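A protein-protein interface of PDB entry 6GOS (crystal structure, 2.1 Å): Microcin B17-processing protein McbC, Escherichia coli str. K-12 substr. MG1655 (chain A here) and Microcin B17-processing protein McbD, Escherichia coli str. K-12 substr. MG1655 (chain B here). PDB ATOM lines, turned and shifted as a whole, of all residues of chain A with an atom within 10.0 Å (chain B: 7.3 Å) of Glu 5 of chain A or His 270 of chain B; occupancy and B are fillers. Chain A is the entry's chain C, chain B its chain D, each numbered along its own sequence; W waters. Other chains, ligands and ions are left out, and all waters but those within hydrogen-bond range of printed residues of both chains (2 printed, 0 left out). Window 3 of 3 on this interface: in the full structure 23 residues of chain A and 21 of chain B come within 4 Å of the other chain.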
ATOM      1  N   SER A   2      18.495  25.934  26.846  1.00  0.00           N
ATOM      2  CA  SER A   2      17.858  24.685  27.413  1.00  0.00           C
ATOM      3  C   SER A   2      16.860  24.065  26.419  1.00  0.00           C
ATOM      4  O   SER A   2      17.041  22.909  26.021  1.00  0.00           O
ATOM      5  CB  SER A   2      17.211  24.953  28.769  1.00  0.00           C
ATOM      6  N   LYS A   3      15.839  24.828  26.003  1.00  0.00           N
ATOM      7  CA  LYS A   3      15.040  24.484  24.797  1.00  0.00           C
ATOM      8  C   LYS A   3      15.899  24.607  23.515  1.00  0.00           C
ATOM      9  O   LYS A   3      15.574  24.032  22.483  1.00  0.00           O
ATOM     10  CB  LYS A   3      13.811  25.389  24.662  1.00  0.00           C
ATOM     11  N   HIS A   4      16.985  25.375  23.591  1.00  0.00           N
ATOM     12  CA  HIS A   4      17.879  25.631  22.464  1.00  0.00           C
ATOM     13  C   HIS A   4      19.255  24.940  22.636  1.00  0.00           C
ATOM     14  O   HIS A   4      20.228  25.327  21.988  1.00  0.00           O
ATOM     15  CB  HIS A   4      18.081  27.156  22.304  1.00  0.00           C
ATOM     16  CG  HIS A   4      16.837  27.972  22.511  1.00  0.00           C
ATOM     17  ND1 HIS A   4      15.903  28.176  21.517  1.00  0.00           N
ATOM     18  CD2 HIS A   4      16.379  28.641  23.598  1.00  0.00           C
ATOM     19  CE1 HIS A   4      14.915  28.919  21.986  1.00  0.00           C
ATOM     20  NE2 HIS A   4      15.173  29.210  23.249  1.00  0.00           N
ATOM     21  N   GLU A   5      19.325  23.910  23.480  1.00  0.00           N
ATOM     22  CA  GLU A   5      20.599  23.320  23.878  1.00  0.00           C
ATOM     23  C   GLU A   5      21.237  22.581  22.734  1.00  0.00           C
ATOM     24  O   GLU A   5      20.570  21.842  22.061  1.00  0.00           O
ATOM     25  CB  GLU A   5      20.428  22.323  25.034  1.00  0.00           C
ATOM     26  CG  GLU A   5      21.753  21.854  25.648  1.00  0.00           C
ATOM     27  CD  GLU A   5      21.591  20.820  26.748  1.00  0.00           C
ATOM     28  OE1 GLU A   5      20.446  20.416  27.047  1.00  0.00           O
ATOM     29  OE2 GLU A   5      22.625  20.399  27.306  1.00  0.00           O
ATOM     30  N   LEU A   6      22.542  22.779  22.571  1.00  0.00           N
ATOM     31  CA  LEU A   6      23.395  22.030  21.662  1.00  0.00           C
ATOM     32  C   LEU A   6      24.502  21.378  22.502  1.00  0.00           C
ATOM     33  O   LEU A   6      25.165  22.065  23.304  1.00  0.00           O
ATOM     34  CB  LEU A   6      24.044  22.986  20.664  1.00  0.00           C
ATOM     35  CG  LEU A   6      25.218  22.456  19.843  1.00  0.00           C
ATOM     36  CD1 LEU A   6      24.743  21.382  18.869  1.00  0.00           C
ATOM     37  CD2 LEU A   6      25.863  23.616  19.119  1.00  0.00           C
ATOM     38  N   SER A   7      24.712  20.074  22.303  1.00  0.00           N
ATOM     39  CA  SER A   7      25.804  19.358  22.954  1.00  0.00           C
ATOM     40  C   SER A   7      27.087  19.536  22.147  1.00  0.00           C
ATOM     41  O   SER A   7      27.084  19.392  20.920  1.00  0.00           O
ATOM     42  CB  SER A   7      25.509  17.859  23.049  1.00  0.00           C
ATOM     43  OG  SER A   7      26.625  17.183  23.634  1.00  0.00           O
ATOM     44  N   LEU A   8      28.189  19.795  22.833  1.00  0.00           N
ATOM     45  CA  LEU A   8      29.487  19.879  22.171  1.00  0.00           C
ATOM     46  C   LEU A   8      29.961  18.534  21.574  1.00  0.00           C
ATOM     47  O   LEU A   8      30.872  18.522  20.743  1.00  0.00           O
ATOM     48  CB  LEU A   8      30.536  20.438  23.136  1.00  0.00           C
ATOM     49  CG  LEU A   8      30.249  21.891  23.495  1.00  0.00           C
ATOM     50  CD1 LEU A   8      31.129  22.333  24.639  1.00  0.00           C
ATOM     51  CD2 LEU A   8      30.414  22.803  22.288  1.00  0.00           C
ATOM     52  N   VAL A   9      29.343  17.422  21.979  1.00  0.00           N
ATOM     53  CA  VAL A   9      29.653  16.111  21.367  1.00  0.00           C
ATOM     54  C   VAL A   9      29.324  16.134  19.868  1.00  0.00           C
ATOM     55  O   VAL A   9      30.039  15.538  19.080  1.00  0.00           O
ATOM     56  CB  VAL A   9      28.906  14.926  22.052  1.00  0.00           C
ATOM     57  CG1 VAL A   9      29.330  13.584  21.439  1.00  0.00           C
ATOM     58  CG2 VAL A   9      29.164  14.886  23.561  1.00  0.00           C
ATOM     59  N   GLU A  10      28.244  16.826  19.489  1.00  0.00           N
ATOM     60  CA  GLU A  10      27.824  16.955  18.073  1.00  0.00           C
ATOM     61  C   GLU A  10      28.813  17.794  17.291  1.00  0.00           C
ATOM     62  O   GLU A  10      29.122  17.494  16.132  1.00  0.00           O
ATOM     63  CB  GLU A  10      26.462  17.649  17.941  1.00  0.00           C
ATOM     64  CG  GLU A  10      25.290  16.943  18.601  1.00  0.00           C
ATOM     65  CD  GLU A  10      24.769  15.740  17.828  1.00  0.00           C
ATOM     66  OE1 GLU A  10      25.304  15.394  16.740  1.00  0.00           O
ATOM     67  OE2 GLU A  10      23.796  15.132  18.332  1.00  0.00           O
ATOM     68  N   VAL A  11      29.258  18.882  17.919  1.00  0.00           N
ATOM     69  CA  VAL A  11      30.231  19.775  17.322  1.00  0.00           C
ATOM     70  C   VAL A  11      31.562  19.074  17.049  1.00  0.00           C
ATOM     71  O   VAL A  11      32.121  19.225  15.966  1.00  0.00           O
ATOM     72  CB  VAL A  11      30.444  21.048  18.180  1.00  0.00           C
ATOM     73  CG1 VAL A  11      31.611  21.881  17.650  1.00  0.00           C
ATOM     74  CG2 VAL A  11      29.184  21.884  18.177  1.00  0.00           C
ATOM     75  N   VAL A 116      14.695  33.402  18.166  1.00  0.00           N
ATOM     76  CA  VAL A 116      16.063  32.896  18.313  1.00  0.00           C
ATOM     77  C   VAL A 116      17.094  33.820  17.649  1.00  0.00           C
ATOM     78  O   VAL A 116      18.291  33.472  17.562  1.00  0.00           O
ATOM     79  CB  VAL A 116      16.201  31.421  17.854  1.00  0.00           C
ATOM     80  CG1 VAL A 116      15.199  30.552  18.614  1.00  0.00           C
ATOM     81  CG2 VAL A 116      16.019  31.263  16.344  1.00  0.00           C
ATOM     82  N   ARG A 118      19.341  37.294  17.534  1.00  0.00           N
ATOM     83  CA  ARG A 118      20.016  38.168  18.498  1.00  0.00           C
ATOM     84  C   ARG A 118      20.322  39.530  17.889  1.00  0.00           C
ATOM     85  O   ARG A 118      20.301  39.689  16.669  1.00  0.00           O
ATOM     86  CB  ARG A 118      21.314  37.509  18.953  1.00  0.00           C
ATOM     87  CG  ARG A 118      21.112  36.100  19.461  1.00  0.00           C
ATOM     88  CD  ARG A 118      22.411  35.521  19.980  1.00  0.00           C
ATOM     89  NE  ARG A 118      22.371  34.059  19.968  1.00  0.00           N
ATOM     90  CZ  ARG A 118      23.187  33.265  20.650  1.00  0.00           C
ATOM     91  NH1 ARG A 118      24.164  33.754  21.415  1.00  0.00           N
ATOM     92  NH2 ARG A 118      23.022  31.956  20.549  1.00  0.00           N
ATOM     93  N   GLU A 130      30.581  32.846  24.285  1.00  0.00           N
ATOM     94  CA  GLU A 130      29.737  32.741  25.468  1.00  0.00           C
ATOM     95  C   GLU A 130      30.028  33.905  26.393  1.00  0.00           C
ATOM     96  O   GLU A 130      31.192  34.341  26.494  1.00  0.00           O
ATOM     97  CB  GLU A 130      30.031  31.446  26.202  1.00  0.00           C
ATOM     98  CG  GLU A 130      29.734  30.190  25.399  1.00  0.00           C
ATOM     99  CD  GLU A 130      28.272  30.006  24.999  1.00  0.00           C
ATOM    100  OE1 GLU A 130      27.337  30.603  25.601  1.00  0.00           O
ATOM    101  OE2 GLU A 130      28.055  29.209  24.075  1.00  0.00           O
ATOM    102  N   HIS A 151      26.500  32.185  33.819  1.00  0.00           N
ATOM    103  CA  HIS A 151      26.609  32.091  32.371  1.00  0.00           C
ATOM    104  C   HIS A 151      25.281  32.579  31.781  1.00  0.00           C
ATOM    105  O   HIS A 151      24.217  32.014  32.104  1.00  0.00           O
ATOM    106  CB  HIS A 151      26.905  30.646  32.011  1.00  0.00           C
ATOM    107  CG  HIS A 151      26.876  30.343  30.547  1.00  0.00           C
ATOM    108  ND1 HIS A 151      26.394  29.149  30.053  1.00  0.00           N
ATOM    109  CD2 HIS A 151      27.268  31.063  29.473  1.00  0.00           C
ATOM    110  CE1 HIS A 151      26.491  29.148  28.736  1.00  0.00           C
ATOM    111  NE2 HIS A 151      27.030  30.292  28.358  1.00  0.00           N
ATOM    112  N   LEU A 153      22.452  32.919  29.136  1.00  0.00           N
ATOM    113  CA  LEU A 153      21.897  32.152  28.033  1.00  0.00           C
ATOM    114  C   LEU A 153      21.052  33.134  27.236  1.00  0.00           C
ATOM    115  O   LEU A 153      19.919  33.423  27.636  1.00  0.00           O
ATOM    116  CB  LEU A 153      21.056  30.989  28.550  1.00  0.00           C
ATOM    117  CG  LEU A 153      21.717  30.015  29.522  1.00  0.00           C
ATOM    118  CD1 LEU A 153      20.762  28.885  29.909  1.00  0.00           C
ATOM    119  CD2 LEU A 153      22.979  29.435  28.909  1.00  0.00           C
ATOM    120  N   LEU A 155      19.321  33.182  24.447  1.00  0.00           N
ATOM    121  CA  LEU A 155      18.077  32.767  23.809  1.00  0.00           C
ATOM    122  C   LEU A 155      17.019  32.388  24.819  1.00  0.00           C
ATOM    123  O   LEU A 155      15.872  32.781  24.658  1.00  0.00           O
ATOM    124  CB  LEU A 155      18.329  31.594  22.856  1.00  0.00           C
ATOM    125  CG  LEU A 155      19.235  31.929  21.682  1.00  0.00           C
ATOM    126  CD1 LEU A 155      19.392  30.722  20.766  1.00  0.00           C
ATOM    127  CD2 LEU A 155      18.677  33.140  20.932  1.00  0.00           C
ATOM    128  N   SER A 156      17.403  31.620  25.846  1.00  0.00           N
ATOM    129  CA  SER A 156      16.518  31.325  26.985  1.00  0.00           C
ATOM    130  C   SER A 156      16.272  32.569  27.832  1.00  0.00           C
ATOM    131  O   SER A 156      15.252  32.665  28.490  1.00  0.00           O
ATOM    132  CB  SER A 156      17.120  30.265  27.901  1.00  0.00           C
ATOM    133  OG  SER A 156      17.453  29.089  27.207  1.00  0.00           O
ATOM    134  N   GLU A 160      22.635  30.871  34.160  1.00  0.00           N
ATOM    135  CA  GLU A 160      23.005  29.554  34.640  1.00  0.00           C
ATOM    136  C   GLU A 160      24.127  29.734  35.694  1.00  0.00           C
ATOM    137  O   GLU A 160      25.111  30.380  35.399  1.00  0.00           O
ATOM    138  CB  GLU A 160      23.469  28.721  33.430  1.00  0.00           C
ATOM    139  CG  GLU A 160      23.888  27.287  33.693  1.00  0.00           C
ATOM    140  CD  GLU A 160      24.465  26.607  32.454  1.00  0.00           C
ATOM    141  OE1 GLU A 160      24.986  27.289  31.536  1.00  0.00           O
ATOM    142  OE2 GLU A 160      24.415  25.369  32.401  1.00  0.00           O
ATOM    143  N   LYS A 197      33.594  25.159  18.574  1.00  0.00           N
ATOM    144  CA  LYS A 197      32.420  25.801  17.984  1.00  0.00           C
ATOM    145  C   LYS A 197      32.825  26.852  16.942  1.00  0.00           C
ATOM    146  O   LYS A 197      32.166  27.015  15.922  1.00  0.00           O
ATOM    147  CB  LYS A 197      31.617  26.451  19.086  1.00  0.00           C
ATOM    148  CG  LYS A 197      30.269  26.934  18.664  1.00  0.00           C
ATOM    149  CD  LYS A 197      29.208  25.902  18.844  1.00  0.00           C
ATOM    150  CE  LYS A 197      27.867  26.607  18.821  1.00  0.00           C
ATOM    151  NZ  LYS A 197      27.320  26.693  17.442  1.00  0.00           N
ATOM    152  N   GLU B 208      18.290  19.104  40.207  1.00  0.00           N
ATOM    153  CA  GLU B 208      17.372  18.738  39.125  1.00  0.00           C
ATOM    154  C   GLU B 208      16.224  17.816  39.612  1.00  0.00           C
ATOM    155  O   GLU B 208      15.118  17.886  39.093  1.00  0.00           O
ATOM    156  CB  GLU B 208      18.138  18.063  37.995  1.00  0.00           C
ATOM    157  CG  GLU B 208      17.359  17.957  36.685  1.00  0.00           C
ATOM    158  CD  GLU B 208      17.424  19.193  35.802  1.00  0.00           C
ATOM    159  OE1 GLU B 208      18.265  20.098  36.053  1.00  0.00           O
ATOM    160  OE2 GLU B 208      16.635  19.231  34.820  1.00  0.00           O
ATOM    161  N   ILE B 236      10.116  20.174  32.362  1.00  0.00           N
ATOM    162  CA  ILE B 236      11.065  20.469  31.257  1.00  0.00           C
ATOM    163  C   ILE B 236      12.322  19.592  31.207  1.00  0.00           C
ATOM    164  O   ILE B 236      13.064  19.673  30.249  1.00  0.00           O
ATOM    165  CB  ILE B 236      11.505  21.961  31.217  1.00  0.00           C
ATOM    166  CG1 ILE B 236      12.528  22.274  32.332  1.00  0.00           C
ATOM    167  CG2 ILE B 236      10.287  22.883  31.247  1.00  0.00           C
ATOM    168  CD1 ILE B 236      12.737  23.750  32.629  1.00  0.00           C
ATOM    169  N   SER B 237      12.576  18.790  32.239  1.00  0.00           N
ATOM    170  CA  SER B 237      13.673  17.818  32.210  1.00  0.00           C
ATOM    171  C   SER B 237      13.351  16.693  31.216  1.00  0.00           C
ATOM    172  O   SER B 237      12.251  16.157  31.231  1.00  0.00           O
ATOM    173  CB  SER B 237      13.911  17.209  33.602  1.00  0.00           C
ATOM    174  OG  SER B 237      14.224  18.196  34.572  1.00  0.00           O
ATOM    175  N   ARG B 238      14.308  16.345  30.359  1.00  0.00           N
ATOM    176  CA  ARG B 238      14.141  15.239  29.419  1.00  0.00           C
ATOM    177  C   ARG B 238      14.354  13.895  30.097  1.00  0.00           C
ATOM    178  O   ARG B 238      13.630  12.941  29.801  1.00  0.00           O
ATOM    179  CB  ARG B 238      15.080  15.386  28.212  1.00  0.00           C
ATOM    180  CG  ARG B 238      14.658  16.454  27.204  1.00  0.00           C
ATOM    181  CD  ARG B 238      15.233  17.838  27.509  1.00  0.00           C
ATOM    182  NE  ARG B 238      15.137  18.757  26.355  1.00  0.00           N
ATOM    183  CZ  ARG B 238      15.840  19.889  26.182  1.00  0.00           C
ATOM    184  NH1 ARG B 238      16.753  20.298  27.070  1.00  0.00           N
ATOM    185  NH2 ARG B 238      15.640  20.626  25.085  1.00  0.00           N
ATOM    186  N   ILE B 239      15.334  13.818  31.001  1.00  0.00           N
ATOM    187  CA  ILE B 239      15.590  12.606  31.782  1.00  0.00           C
ATOM    188  C   ILE B 239      14.775  12.628  33.086  1.00  0.00           C
ATOM    189  O   ILE B 239      15.017  13.447  33.980  1.00  0.00           O
ATOM    190  CB  ILE B 239      17.086  12.423  32.096  1.00  0.00           C
ATOM    191  CG1 ILE B 239      17.938  12.457  30.809  1.00  0.00           C
ATOM    192  CG2 ILE B 239      17.329  11.135  32.890  1.00  0.00           C
ATOM    193  CD1 ILE B 239      17.525  11.458  29.749  1.00  0.00           C
ATOM    194  N   GLN B 264      27.021   9.305  32.795  1.00  0.00           N
ATOM    195  CA  GLN B 264      27.204   8.801  31.452  1.00  0.00           C
ATOM    196  C   GLN B 264      25.879   8.355  30.808  1.00  0.00           C
ATOM    197  O   GLN B 264      25.608   8.711  29.680  1.00  0.00           O
ATOM    198  CB  GLN B 264      28.247   7.674  31.458  1.00  0.00           C
ATOM    199  CG  GLN B 264      28.380   6.965  30.127  1.00  0.00           C
ATOM    200  CD  GLN B 264      29.602   6.085  30.036  1.00  0.00           C
ATOM    201  OE1 GLN B 264      30.401   6.231  29.106  1.00  0.00           O
ATOM    202  NE2 GLN B 264      29.762   5.165  30.989  1.00  0.00           N
ATOM    203  N   SER B 265      25.044   7.607  31.525  1.00  0.00           N
ATOM    204  CA  SER B 265      23.764   7.164  30.961  1.00  0.00           C
ATOM    205  C   SER B 265      22.809   8.303  30.825  1.00  0.00           C
ATOM    206  O   SER B 265      22.084   8.377  29.858  1.00  0.00           O
ATOM    207  CB  SER B 265      23.113   6.077  31.812  1.00  0.00           C
ATOM    208  OG  SER B 265      23.718   4.854  31.510  1.00  0.00           O
ATOM    209  N   TYR B 266      22.805   9.172  31.824  1.00  0.00           N
ATOM    210  CA  TYR B 266      21.972  10.363  31.845  1.00  0.00           C
ATOM    211  C   TYR B 266      22.255  11.186  30.609  1.00  0.00           C
ATOM    212  O   TYR B 266      21.334  11.518  29.859  1.00  0.00           O
ATOM    213  CB  TYR B 266      22.294  11.162  33.110  1.00  0.00           C
ATOM    214  CG  TYR B 266      21.486  12.405  33.319  1.00  0.00           C
ATOM    215  CD1 TYR B 266      21.766  13.574  32.609  1.00  0.00           C
ATOM    216  CD2 TYR B 266      20.493  12.442  34.262  1.00  0.00           C
ATOM    217  CE1 TYR B 266      21.033  14.729  32.813  1.00  0.00           C
ATOM    218  CE2 TYR B 266      19.771  13.595  34.482  1.00  0.00           C
ATOM    219  CZ  TYR B 266      20.030  14.735  33.743  1.00  0.00           C
ATOM    220  OH  TYR B 266      19.300  15.888  33.963  1.00  0.00           O
ATOM    221  N   ILE B 267      23.534  11.500  30.378  1.00  0.00           N
ATOM    222  CA  ILE B 267      23.885  12.415  29.303  1.00  0.00           C
ATOM    223  C   ILE B 267      23.722  11.802  27.904  1.00  0.00           C
ATOM    224  O   ILE B 267      23.259  12.496  27.002  1.00  0.00           O
ATOM    225  CB  ILE B 267      25.284  13.060  29.517  1.00  0.00           C
ATOM    226  CG1 ILE B 267      25.429  14.322  28.659  1.00  0.00           C
ATOM    227  CG2 ILE B 267      26.410  12.097  29.211  1.00  0.00           C
ATOM    228  CD1 ILE B 267      24.584  15.493  29.129  1.00  0.00           C
ATOM    229  N   CYS B 268      24.064  10.521  27.729  1.00  0.00           N
ATOM    230  CA  CYS B 268      23.893   9.863  26.439  1.00  0.00           C
ATOM    231  C   CYS B 268      22.459   9.845  26.013  1.00  0.00           C
ATOM    232  O   CYS B 268      22.167  10.187  24.890  1.00  0.00           O
ATOM    233  CB  CYS B 268      24.450   8.451  26.432  1.00  0.00           C
ATOM    234  SG  CYS B 268      26.239   8.535  26.470  1.00  0.00           S
ATOM    235  N   LEU B 269      21.556   9.499  26.925  1.00  0.00           N
ATOM    236  CA  LEU B 269      20.125   9.541  26.614  1.00  0.00           C
ATOM    237  C   LEU B 269      19.639  10.978  26.410  1.00  0.00           C
ATOM    238  O   LEU B 269      18.889  11.246  25.478  1.00  0.00           O
ATOM    239  CB  LEU B 269      19.283   8.810  27.681  1.00  0.00           C
ATOM    240  CG  LEU B 269      17.765   8.744  27.433  1.00  0.00           C
ATOM    241  CD1 LEU B 269      17.424   8.306  26.014  1.00  0.00           C
ATOM    242  CD2 LEU B 269      17.095   7.838  28.462  1.00  0.00           C
ATOM    243  N   HIS B 270      20.077  11.904  27.262  1.00  0.00           N
ATOM    244  CA  HIS B 270      19.704  13.325  27.122  1.00  0.00           C
ATOM    245  C   HIS B 270      20.084  13.840  25.741  1.00  0.00           C
ATOM    246  O   HIS B 270      19.256  14.446  25.061  1.00  0.00           O
ATOM    247  CB  HIS B 270      20.348  14.182  28.214  1.00  0.00           C
ATOM    248  CG  HIS B 270      20.021  15.637  28.110  1.00  0.00           C
ATOM    249  ND1 HIS B 270      18.883  16.190  28.663  1.00  0.00           N
ATOM    250  CD2 HIS B 270      20.673  16.654  27.494  1.00  0.00           C
ATOM    251  CE1 HIS B 270      18.864  17.489  28.413  1.00  0.00           C
ATOM    252  NE2 HIS B 270      19.933  17.794  27.698  1.00  0.00           N
ATOM    253  N   ASN B 271      21.310  13.559  25.318  1.00  0.00           N
ATOM    254  CA  ASN B 271      21.801  14.019  24.016  1.00  0.00           C
ATOM    255  C   ASN B 271      21.094  13.356  22.816  1.00  0.00           C
ATOM    256  O   ASN B 271      20.848  13.993  21.778  1.00  0.00           O
ATOM    257  CB  ASN B 271      23.317  13.849  23.932  1.00  0.00           C
ATOM    258  CG  ASN B 271      24.073  14.912  24.735  1.00  0.00           C
ATOM    259  OD1 ASN B 271      23.509  15.957  25.101  1.00  0.00           O
ATOM    260  ND2 ASN B 271      25.357  14.656  25.000  1.00  0.00           N
ATOM    261  N   PHE B 272      20.750  12.084  22.975  1.00  0.00           N
ATOM    262  CA  PHE B 272      19.916  11.399  21.997  1.00  0.00           C
ATOM    263  C   PHE B 272      18.565  12.129  21.835  1.00  0.00           C
ATOM    264  O   PHE B 272      18.106  12.386  20.708  1.00  0.00           O
ATOM    265  CB  PHE B 272      19.717   9.936  22.418  1.00  0.00           C
ATOM    266  CG  PHE B 272      18.967   9.122  21.420  1.00  0.00           C
ATOM    267  CD1 PHE B 272      17.577   9.098  21.428  1.00  0.00           C
ATOM    268  CD2 PHE B 272      19.649   8.396  20.445  1.00  0.00           C
ATOM    269  CE1 PHE B 272      16.878   8.361  20.486  1.00  0.00           C
ATOM    270  CE2 PHE B 272      18.949   7.658  19.498  1.00  0.00           C
ATOM    271  CZ  PHE B 272      17.573   7.638  19.529  1.00  0.00           C
ATOM    272  N   LEU B 273      17.957  12.481  22.967  1.00  0.00           N
ATOM    273  CA  LEU B 273      16.650  13.139  22.977  1.00  0.00           C
ATOM    274  C   LEU B 273      16.650  14.600  22.488  1.00  0.00           C
ATOM    275  O   LEU B 273      15.699  15.018  21.848  1.00  0.00           O
ATOM    276  CB  LEU B 273      16.011  13.035  24.366  1.00  0.00           C
ATOM    277  CG  LEU B 273      15.587  11.618  24.769  1.00  0.00           C
ATOM    278  CD1 LEU B 273      15.468  11.519  26.275  1.00  0.00           C
ATOM    279  CD2 LEU B 273      14.277  11.213  24.104  1.00  0.00           C
ATOM    280  N   ILE B 274      17.695  15.376  22.770  1.00  0.00           N
ATOM    281  CA  ILE B 274      17.774  16.752  22.229  1.00  0.00           C
ATOM    282  C   ILE B 274      18.347  16.775  20.804  1.00  0.00           C
ATOM    283  O   ILE B 274      18.163  17.749  20.098  1.00  0.00           O
ATOM    284  CB  ILE B 274      18.534  17.738  23.154  1.00  0.00           C
ATOM    285  CG1 ILE B 274      20.041  17.418  23.228  1.00  0.00           C
ATOM    286  CG2 ILE B 274      17.900  17.753  24.539  1.00  0.00           C
ATOM    287  CD1 ILE B 274      20.843  18.463  23.967  1.00  0.00           C
ATOM    288  N   GLY B 275      19.056  15.715  20.403  1.00  0.00           N
ATOM    289  CA  GLY B 275      19.377  15.472  18.986  1.00  0.00           C
ATOM    290  C   GLY B 275      18.171  15.221  18.069  1.00  0.00           C
ATOM    291  O   GLY B 275      18.277  15.369  16.852  1.00  0.00           O
ATOM    292  N   GLY B 276      17.028  14.835  18.644  1.00  0.00           N
ATOM    293  CA  GLY B 276      15.825  14.515  17.867  1.00  0.00           C
ATOM    294  C   GLY B 276      15.944  13.214  17.078  1.00  0.00           C
ATOM    295  O   GLY B 276      15.176  12.980  16.144  1.00  0.00           O
ATOM    296  N   ASN B 294      12.511   5.441  30.925  1.00  0.00           N
ATOM    297  CA  ASN B 294      12.778   6.842  31.319  1.00  0.00           C
ATOM    298  C   ASN B 294      11.469   7.525  31.717  1.00  0.00           C
ATOM    299  O   ASN B 294      10.870   8.284  30.966  1.00  0.00           O
ATOM    300  CB  ASN B 294      13.553   7.624  30.228  1.00  0.00           C
ATOM    301  CG  ASN B 294      13.697   9.108  30.549  1.00  0.00           C
ATOM    302  OD1 ASN B 294      13.944   9.505  31.699  1.00  0.00           O
ATOM    303  ND2 ASN B 294      13.506   9.937  29.538  1.00  0.00           N
HETATM  304  O   HOH W   1      26.404  17.504  26.270  1.00  0.00           O
HETATM  305  O   HOH W   2      22.726  15.883  20.780  1.00  0.00           O
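The backbone carbonyl oxygen (O) of Ser 2 of chain A sits at hydrogen-bond distance from the guanidinium group (NH1) of Arg 238 of chain B (2.8 Å). OE1 of Glu 5 of chain A lies within salt-bridge range of NH1 of Arg 238 of chain B, 3.7 Å away. NE2 of His 270 of chain B lies within hydrogen-bond range of OE1 of Glu 5 of chain A (2.7 Å). The side-chain hydroxyl of Ser 7 of chain A lies within hydrogen-bond range of the side-chain amide nitrogen of Asn 271 of chain B (3.1 Å).
The backbone NH of Ser 2 of chain A is in hydrogen-bond range of the side-chain hydroxyl of Ser 156 of chain A, 3.3 Å away. The side-chain hydroxyl of Ser 7 of chain A lies close to the backbone NH of Val 9 of chain A, 3.2 Å away. ND2 of Asn 294 of chain B lies within hydrogen-bond range of O of Arg 238 of chain B (3.0 Å).
Among the printed residues, pairs that only touch across the chains: Lys 3 of chain A with Arg 238 of chain B (3.9 Å) and Glu 5 of chain A with Ile 274 of chain B (3.7 Å).
Of the printed residues of chain B, Ser 2 of chain A touches Arg 238. Of the printed residues of chain B, Lys 3 of chain A touches Arg 238. Of chain B, only Arg 238, His 270 and Ile 274 come within 4 Å of Glu 5 of chain A. No residue of chain A comes within 4 Å of Leu 269 of chain B. His 270 of chain B touches just one residue of chain A: Glu 5. Ile 274 of chain B touches just one residue of chain A: Glu 5. The nearest residue of chain B that does not touch Glu 5 of chain A is Asn 271 of chain B (5.0 Å). The nearest residue of chain A that does not touch His 270 of chain B is Ser 2 of chain A (6.1 Å). The nearest printed residue of chain B that does not touch Lys 3 of chain A is Ile 274 of chain B (7.0 Å).
Of the 19 printed residues of chain B, 4 touch a printed residue of chain A. Printed residues of chain B that touch a printed residue of chain A: Arg 238, His 270, Asn 271 and Ile 274. Along chain B the printed residues that touch a printed residue of chain A span positions 238 to 274. Of the 19 printed residues of chain A, 4 touch a printed residue of chain B. Printed residues of chain A that touch a printed residue of chain B: Ser 2, Lys 3, Glu 5 and Ser 7. Among the printed residues, 6 pairs touch across the chains.
Water W1 bridges the side-chain hydroxyl (OG) of Ser 7 of chain A (2.7 Å) and the side-chain amide nitrogen (ND2) of Asn 271 of chain B (3.3 Å). Water W2 bridges the side-chain carboxylate of Glu 10 of chain A (2.8 Å) and the backbone carbonyl oxygen of Asn 271 of chain B (2.8 Å).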
